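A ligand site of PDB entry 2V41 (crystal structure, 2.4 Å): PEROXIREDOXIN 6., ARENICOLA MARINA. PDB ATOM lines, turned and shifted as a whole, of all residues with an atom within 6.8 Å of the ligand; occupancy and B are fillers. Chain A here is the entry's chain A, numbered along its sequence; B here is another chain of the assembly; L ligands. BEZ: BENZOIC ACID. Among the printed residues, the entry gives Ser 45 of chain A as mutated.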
ATOM      1  N   HIS A  37       6.835 -20.474  -9.590  1.00  0.00           N
ATOM      2  CA  HIS A  37       6.516 -21.115  -8.300  1.00  0.00           C
ATOM      3  C   HIS A  37       5.756 -22.388  -8.552  1.00  0.00           C
ATOM      4  O   HIS A  37       5.204 -22.571  -9.616  1.00  0.00           O
ATOM      5  CB  HIS A  37       5.773 -20.169  -7.348  1.00  0.00           C
ATOM      6  CG  HIS A  37       4.419 -19.758  -7.838  1.00  0.00           C
ATOM      7  ND1 HIS A  37       4.233 -18.697  -8.701  1.00  0.00           N
ATOM      8  CD2 HIS A  37       3.190 -20.249  -7.576  1.00  0.00           C
ATOM      9  CE1 HIS A  37       2.946 -18.565  -8.958  1.00  0.00           C
ATOM     10  NE2 HIS A  37       2.295 -19.499  -8.293  1.00  0.00           N
ATOM     11  N   PRO A  38       5.842 -23.344  -7.646  1.00  0.00           N
ATOM     12  CA  PRO A  38       5.240 -24.645  -7.989  1.00  0.00           C
ATOM     13  C   PRO A  38       3.776 -24.634  -8.304  1.00  0.00           C
ATOM     14  O   PRO A  38       3.364 -25.287  -9.247  1.00  0.00           O
ATOM     15  CB  PRO A  38       5.479 -25.485  -6.716  1.00  0.00           C
ATOM     16  CG  PRO A  38       6.684 -24.922  -6.135  1.00  0.00           C
ATOM     17  CD  PRO A  38       6.552 -23.430  -6.357  1.00  0.00           C
ATOM     18  N   ARG A  39       2.989 -23.930  -7.498  1.00  0.00           N
ATOM     19  CA  ARG A  39       1.527 -24.118  -7.479  1.00  0.00           C
ATOM     20  C   ARG A  39       0.963 -22.967  -6.656  1.00  0.00           C
ATOM     21  O   ARG A  39       1.535 -22.573  -5.640  1.00  0.00           O
ATOM     22  CB  ARG A  39       1.179 -25.460  -6.833  1.00  0.00           C
ATOM     23  CG  ARG A  39      -0.106 -26.093  -7.255  1.00  0.00           C
ATOM     24  CD  ARG A  39      -0.054 -26.723  -8.659  1.00  0.00           C
ATOM     25  NE  ARG A  39      -1.391 -26.990  -9.257  1.00  0.00           N
ATOM     26  CZ  ARG A  39      -2.106 -28.091  -9.045  1.00  0.00           C
ATOM     27  NH1 ARG A  39      -1.637 -29.082  -8.280  1.00  0.00           N
ATOM     28  NH2 ARG A  39      -3.303 -28.228  -9.614  1.00  0.00           N
ATOM     29  N   PHE A  41      -1.989 -21.293  -4.266  1.00  0.00           N
ATOM     30  CA  PHE A  41      -2.714 -21.752  -3.083  1.00  0.00           C
ATOM     31  C   PHE A  41      -1.860 -22.643  -2.192  1.00  0.00           C
ATOM     32  O   PHE A  41      -2.376 -23.589  -1.510  1.00  0.00           O
ATOM     33  CB  PHE A  41      -3.998 -22.474  -3.470  1.00  0.00           C
ATOM     34  CG  PHE A  41      -5.017 -21.596  -4.158  1.00  0.00           C
ATOM     35  CD1 PHE A  41      -5.670 -20.603  -3.478  1.00  0.00           C
ATOM     36  CD2 PHE A  41      -5.354 -21.819  -5.505  1.00  0.00           C
ATOM     37  CE1 PHE A  41      -6.632 -19.836  -4.108  1.00  0.00           C
ATOM     38  CE2 PHE A  41      -6.284 -21.065  -6.128  1.00  0.00           C
ATOM     39  CZ  PHE A  41      -6.946 -20.073  -5.447  1.00  0.00           C
ATOM     40  N   THR A  42      -0.575 -22.341  -2.202  1.00  0.00           N
ATOM     41  CA  THR A  42       0.397 -23.064  -1.388  1.00  0.00           C
ATOM     42  C   THR A  42       1.116 -22.047  -0.554  1.00  0.00           C
ATOM     43  O   THR A  42       1.276 -20.897  -1.003  1.00  0.00           O
ATOM     44  CB  THR A  42       1.421 -23.783  -2.240  1.00  0.00           C
ATOM     45  OG1 THR A  42       1.984 -22.852  -3.164  1.00  0.00           O
ATOM     46  CG2 THR A  42       0.768 -24.963  -2.988  1.00  0.00           C
ATOM     47  N   PRO A  43       1.546 -22.448   0.670  1.00  0.00           N
ATOM     48  CA  PRO A  43       2.028 -21.495   1.695  1.00  0.00           C
ATOM     49  C   PRO A  43       3.314 -20.699   1.395  1.00  0.00           C
ATOM     50  O   PRO A  43       3.281 -19.476   1.524  1.00  0.00           O
ATOM     51  CB  PRO A  43       2.176 -22.353   2.968  1.00  0.00           C
ATOM     52  CG  PRO A  43       2.089 -23.787   2.507  1.00  0.00           C
ATOM     53  CD  PRO A  43       1.470 -23.835   1.173  1.00  0.00           C
ATOM     54  N   VAL A  44       4.411 -21.373   1.068  1.00  0.00           N
ATOM     55  CA  VAL A  44       5.673 -20.706   0.709  1.00  0.00           C
ATOM     56  C   VAL A  44       5.511 -19.791  -0.506  1.00  0.00           C
ATOM     57  O   VAL A  44       5.960 -18.673  -0.499  1.00  0.00           O
ATOM     58  CB  VAL A  44       6.873 -21.704   0.519  1.00  0.00           C
ATOM     59  CG1 VAL A  44       8.071 -21.015  -0.072  1.00  0.00           C
ATOM     60  CG2 VAL A  44       7.276 -22.291   1.873  1.00  0.00           C
ATOM     61  N   SER A  45       4.820 -20.267  -1.530  1.00  0.00           N
ATOM     62  CA  SER A  45       4.582 -19.481  -2.758  1.00  0.00           C
ATOM     63  C   SER A  45       3.875 -18.173  -2.448  1.00  0.00           C
ATOM     64  O   SER A  45       4.174 -17.191  -3.078  1.00  0.00           O
ATOM     65  CB  SER A  45       3.785 -20.287  -3.795  1.00  0.00           C
ATOM     66  OG  SER A  45       4.340 -21.572  -4.037  1.00  0.00           O
ATOM     67  N   THR A  46       2.976 -18.148  -1.459  1.00  0.00           N
ATOM     68  CA  THR A  46       2.240 -16.922  -1.051  1.00  0.00           C
ATOM     69  C   THR A  46       3.128 -15.905  -0.292  1.00  0.00           C
ATOM     70  O   THR A  46       3.027 -14.673  -0.473  1.00  0.00           O
ATOM     71  CB  THR A  46       0.956 -17.270  -0.221  1.00  0.00           C
ATOM     72  OG1 THR A  46       0.186 -18.279  -0.887  1.00  0.00           O
ATOM     73  CG2 THR A  46       0.065 -16.074  -0.055  1.00  0.00           C
ATOM     74  N   GLU A  48       6.389 -15.689  -0.713  1.00  0.00           N
ATOM     75  CA  GLU A  48       7.334 -15.086  -1.705  1.00  0.00           C
ATOM     76  C   GLU A  48       6.716 -14.072  -2.665  1.00  0.00           C
ATOM     77  O   GLU A  48       7.267 -13.026  -2.952  1.00  0.00           O
ATOM     78  CB  GLU A  48       7.969 -16.160  -2.563  1.00  0.00           C
ATOM     79  CG  GLU A  48       8.708 -17.263  -1.860  1.00  0.00           C
ATOM     80  CD  GLU A  48       9.303 -18.245  -2.852  1.00  0.00           C
ATOM     81  OE1 GLU A  48       8.527 -18.854  -3.599  1.00  0.00           O
ATOM     82  OE2 GLU A  48      10.566 -18.356  -2.936  1.00  0.00           O
ATOM     83  N   ASP A 114      10.232 -29.120 -11.193  1.00  0.00           N
ATOM     84  CA  ASP A 114      10.516 -29.459  -9.805  1.00  0.00           C
ATOM     85  C   ASP A 114      10.795 -30.945  -9.726  1.00  0.00           C
ATOM     86  O   ASP A 114      10.114 -31.748 -10.351  1.00  0.00           O
ATOM     87  CB  ASP A 114       9.363 -29.039  -8.858  1.00  0.00           C
ATOM     88  CG  ASP A 114       9.778 -29.077  -7.385  1.00  0.00           C
ATOM     89  OD1 ASP A 114      10.222 -28.055  -6.881  1.00  0.00           O
ATOM     90  OD2 ASP A 114       9.716 -30.127  -6.706  1.00  0.00           O
ATOM     91  N   GLU A 117       7.749 -32.194  -6.724  1.00  0.00           N
ATOM     92  CA  GLU A 117       6.318 -31.821  -6.755  1.00  0.00           C
ATOM     93  C   GLU A 117       5.674 -32.012  -8.099  1.00  0.00           C
ATOM     94  O   GLU A 117       6.142 -31.495  -9.112  1.00  0.00           O
ATOM     95  CB  GLU A 117       6.101 -30.391  -6.288  1.00  0.00           C
ATOM     96  CG  GLU A 117       6.629 -30.200  -4.850  1.00  0.00           C
ATOM     97  CD  GLU A 117       5.947 -31.136  -3.854  1.00  0.00           C
ATOM     98  OE1 GLU A 117       4.708 -31.279  -4.046  1.00  0.00           O
ATOM     99  OE2 GLU A 117       6.647 -31.674  -2.919  1.00  0.00           O
ATOM    100  N   LEU A 125       5.292 -29.856 -12.315  1.00  0.00           N
ATOM    101  CA  LEU A 125       5.159 -28.494 -11.855  1.00  0.00           C
ATOM    102  C   LEU A 125       6.560 -27.883 -11.914  1.00  0.00           C
ATOM    103  O   LEU A 125       7.571 -28.607 -12.005  1.00  0.00           O
ATOM    104  CB  LEU A 125       4.559 -28.418 -10.440  1.00  0.00           C
ATOM    105  CG  LEU A 125       3.189 -29.046 -10.215  1.00  0.00           C
ATOM    106  CD1 LEU A 125       2.687 -29.046  -8.790  1.00  0.00           C
ATOM    107  CD2 LEU A 125       2.166 -28.375 -11.097  1.00  0.00           C
ATOM    108  N   ARG A 128      11.029 -23.190  -7.851  1.00  0.00           N
ATOM    109  CA  ARG A 128      11.240 -21.786  -7.670  1.00  0.00           C
ATOM    110  C   ARG A 128      12.500 -21.325  -8.433  1.00  0.00           C
ATOM    111  O   ARG A 128      13.613 -21.306  -7.911  1.00  0.00           O
ATOM    112  CB  ARG A 128      11.345 -21.494  -6.178  1.00  0.00           C
ATOM    113  CG  ARG A 128      10.224 -22.112  -5.370  1.00  0.00           C
ATOM    114  CD  ARG A 128      10.318 -21.779  -3.872  1.00  0.00           C
ATOM    115  NE  ARG A 128       9.348 -22.626  -3.195  1.00  0.00           N
ATOM    116  CZ  ARG A 128       8.038 -22.454  -3.234  1.00  0.00           C
ATOM    117  NH1 ARG A 128       7.507 -21.393  -3.815  1.00  0.00           N
ATOM    118  NH2 ARG A 128       7.255 -23.347  -2.663  1.00  0.00           N
ATOM    119  N   ALA A 147      10.830 -26.704  -4.495  1.00  0.00           N
ATOM    120  CA  ALA A 147       9.630 -26.328  -3.818  1.00  0.00           C
ATOM    121  C   ALA A 147       9.877 -26.182  -2.317  1.00  0.00           C
ATOM    122  O   ALA A 147       9.156 -25.406  -1.632  1.00  0.00           O
ATOM    123  CB  ALA A 147       8.540 -27.342  -4.069  1.00  0.00           C
ATOM    124  N   THR A 148      10.834 -26.954  -1.773  1.00  0.00           N
ATOM    125  CA  THR A 148      11.062 -26.941  -0.303  1.00  0.00           C
ATOM    126  C   THR A 148      11.580 -25.602   0.255  1.00  0.00           C
ATOM    127  O   THR A 148      11.457 -25.328   1.441  1.00  0.00           O
ATOM    128  CB  THR A 148      12.070 -28.035   0.147  1.00  0.00           C
ATOM    129  OG1 THR A 148      13.373 -27.783  -0.449  1.00  0.00           O
ATOM    130  CG2 THR A 148      11.564 -29.439  -0.202  1.00  0.00           C
ATOM    131  N   VAL B 171       7.960 -30.065   6.158  1.00  0.00           N
ATOM    132  CA  VAL B 171       7.884 -28.606   6.124  1.00  0.00           C
ATOM    133  C   VAL B 171       8.570 -28.007   4.883  1.00  0.00           C
ATOM    134  O   VAL B 171       9.226 -28.702   4.089  1.00  0.00           O
ATOM    135  CB  VAL B 171       8.529 -27.938   7.400  1.00  0.00           C
ATOM    136  CG1 VAL B 171       7.773 -28.374   8.700  1.00  0.00           C
ATOM    137  CG2 VAL B 171      10.086 -28.199   7.427  1.00  0.00           C
ATOM    138  N   ALA B 172       8.367 -26.681   4.730  1.00  0.00           N
ATOM    139  CA  ALA B 172       8.991 -25.922   3.641  1.00  0.00           C
ATOM    140  C   ALA B 172       9.264 -24.591   4.251  1.00  0.00           C
ATOM    141  O   ALA B 172       8.507 -24.159   5.082  1.00  0.00           O
ATOM    142  CB  ALA B 172       8.067 -25.830   2.349  1.00  0.00           C
ATOM    143  N   THR B 173      10.381 -23.976   3.864  1.00  0.00           N
ATOM    144  CA  THR B 173      10.789 -22.752   4.453  1.00  0.00           C
ATOM    145  C   THR B 173      10.401 -21.554   3.584  1.00  0.00           C
ATOM    146  O   THR B 173      10.640 -21.518   2.400  1.00  0.00           O
ATOM    147  CB  THR B 173      12.265 -22.771   4.721  1.00  0.00           C
ATOM    148  OG1 THR B 173      12.951 -22.878   3.489  1.00  0.00           O
ATOM    149  CG2 THR B 173      12.604 -23.943   5.667  1.00  0.00           C
ATOM    150  N   MET B 184       6.585 -23.516   7.007  1.00  0.00           N
ATOM    151  CA  MET B 184       5.263 -23.769   6.552  1.00  0.00           C
ATOM    152  C   MET B 184       5.057 -25.262   6.534  1.00  0.00           C
ATOM    153  O   MET B 184       5.974 -25.991   6.265  1.00  0.00           O
ATOM    154  CB  MET B 184       5.053 -23.176   5.140  1.00  0.00           C
ATOM    155  CG  MET B 184       5.480 -21.745   5.009  1.00  0.00           C
ATOM    156  SD  MET B 184       4.896 -20.593   6.277  1.00  0.00           S
ATOM    157  CE  MET B 184       3.138 -20.484   5.883  1.00  0.00           C
ATOM    158  N   VAL B 185       3.852 -25.705   6.883  1.00  0.00           N
ATOM    159  CA  VAL B 185       3.525 -27.127   6.837  1.00  0.00           C
ATOM    160  C   VAL B 185       3.197 -27.317   5.383  1.00  0.00           C
ATOM    161  O   VAL B 185       2.436 -26.506   4.806  1.00  0.00           O
ATOM    162  CB  VAL B 185       2.318 -27.449   7.713  1.00  0.00           C
ATOM    163  CG1 VAL B 185       1.855 -28.876   7.533  1.00  0.00           C
ATOM    164  CG2 VAL B 185       2.669 -27.144   9.160  1.00  0.00           C
ATOM    165  N   VAL B 186       3.791 -28.339   4.763  1.00  0.00           N
ATOM    166  CA  VAL B 186       3.653 -28.540   3.344  1.00  0.00           C
ATOM    167  C   VAL B 186       2.190 -28.837   3.048  1.00  0.00           C
ATOM    168  O   VAL B 186       1.496 -29.412   3.866  1.00  0.00           O
ATOM    169  CB  VAL B 186       4.583 -29.645   2.810  1.00  0.00           C
ATOM    170  CG1 VAL B 186       6.040 -29.269   3.094  1.00  0.00           C
ATOM    171  CG2 VAL B 186       4.221 -31.041   3.360  1.00  0.00           C
ATOM    172  N   PRO B 187       1.725 -28.467   1.843  1.00  0.00           N
ATOM    173  CA  PRO B 187       0.313 -28.599   1.547  1.00  0.00           C
ATOM    174  C   PRO B 187      -0.185 -30.062   1.558  1.00  0.00           C
ATOM    175  O   PRO B 187      -1.360 -30.274   1.751  1.00  0.00           O
ATOM    176  CB  PRO B 187       0.190 -27.916   0.192  1.00  0.00           C
ATOM    177  CG  PRO B 187       1.529 -27.969  -0.406  1.00  0.00           C
ATOM    178  CD  PRO B 187       2.482 -27.919   0.699  1.00  0.00           C
ATOM    179  N   GLY B 188       0.691 -31.049   1.430  1.00  0.00           N
ATOM    180  CA  GLY B 188       0.258 -32.453   1.370  1.00  0.00           C
ATOM    181  C   GLY B 188       0.002 -33.181   2.697  1.00  0.00           C
ATOM    182  O   GLY B 188      -0.404 -34.361   2.683  1.00  0.00           O
ATOM    183  N   TYR B 212      -4.567 -23.456   3.676  1.00  0.00           N
ATOM    184  CA  TYR B 212      -3.236 -23.835   3.270  1.00  0.00           C
ATOM    185  C   TYR B 212      -2.116 -23.037   3.956  1.00  0.00           C
ATOM    186  O   TYR B 212      -0.968 -23.502   4.025  1.00  0.00           O
ATOM    187  CB  TYR B 212      -3.095 -23.750   1.734  1.00  0.00           C
ATOM    188  CG  TYR B 212      -3.119 -22.334   1.194  1.00  0.00           C
ATOM    189  CD1 TYR B 212      -1.986 -21.536   1.227  1.00  0.00           C
ATOM    190  CD2 TYR B 212      -4.255 -21.796   0.660  1.00  0.00           C
ATOM    191  CE1 TYR B 212      -1.991 -20.247   0.751  1.00  0.00           C
ATOM    192  CE2 TYR B 212      -4.267 -20.509   0.200  1.00  0.00           C
ATOM    193  CZ  TYR B 212      -3.139 -19.749   0.251  1.00  0.00           C
ATOM    194  OH  TYR B 212      -3.152 -18.482  -0.218  1.00  0.00           O
HETATM  195  C   BEZ L   1       4.668 -24.239  -0.774  1.00  0.00           C
HETATM  196  O1  BEZ L   1       4.519 -24.236   0.469  1.00  0.00           O
HETATM  197  O2  BEZ L   1       4.621 -23.223  -1.501  1.00  0.00           O
HETATM  198  C1  BEZ L   1       4.873 -25.521  -1.427  1.00  0.00           C
HETATM  199  C2  BEZ L   1       4.522 -25.666  -2.771  1.00  0.00           C
HETATM  200  C3  BEZ L   1       4.709 -26.914  -3.345  1.00  0.00           C
HETATM  201  C4  BEZ L   1       5.182 -27.976  -2.587  1.00  0.00           C
HETATM  202  C5  BEZ L   1       5.509 -27.816  -1.251  1.00  0.00           C
HETATM  203  C6  BEZ L   1       5.353 -26.574  -0.677  1.00  0.00           C
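O of Ala 147 lies within hydrogen-bond range of NH2 of Arg 128 (3.0 Å). OG1 of Thr 42 lies within hydrogen-bond range of O of Arg 39 (2.5 Å). The guanidinium group (NH1) of Arg 128 is in salt-bridge range of the side-chain carboxylate (OE1) of Glu 48. The backbone NH of Glu 117 is in hydrogen-bond range of the side-chain carboxylate of Asp 114 (2.9 Å). OG of Ser 45 lies within hydrogen-bond range of NH1 of Arg 128. The backbone NH (N) of Ala 147 lies within hydrogen-bond range of the side-chain carboxylate (OD1) of Asp 114 (2.8 Å). The side-chain hydroxyl (OG) of Ser 45 sits at hydrogen-bond distance from the backbone carbonyl oxygen (O) of Arg 39, 3.4 Å away. The side-chain hydroxyl (OG) of Ser 45 is in hydrogen-bond range of the side-chain hydroxyl (OG1) of Thr 42 (2.8 Å).
The guanidinium group (NH2) of Arg 128 is in salt-bridge range of an oxygen (O2) of the ligand (2.9 Å). O2 of the ligand lies within hydrogen-bond range of OG1 of Thr 42, at 3.1 Å. N of Val 44 is in hydrogen-bond range of O1 of the ligand (2.9 Å). O2 of the ligand lies within hydrogen-bond range of N of Ser 45 (3.0 Å). O2 of the ligand is in hydrogen-bond range of OG of Ser 45, at 3.0 Å.
O1 of the ligand lies close to N of Pro 43. Merely in contact with the ligand: Pro 187 of chain B (3.5 Å), Glu 117 (3.5 Å), Ala 147 (3.7 Å) and Pro 38 (3.7 Å). Hydrophobic or aromatic side chains that line the ligand: Pro 38, Pro 43, Val 44, Ala 147 and Pro 187 of chain B. Within 4 Å of the ligand: Pro 38, Thr 42, Pro 43, Val 44, Ser 45, Glu 117, Arg 128, Ala 147 and Pro 187 of chain B. The nearest printed residue that does not touch the ligand is Ala 172 of chain B (4.1 Å).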
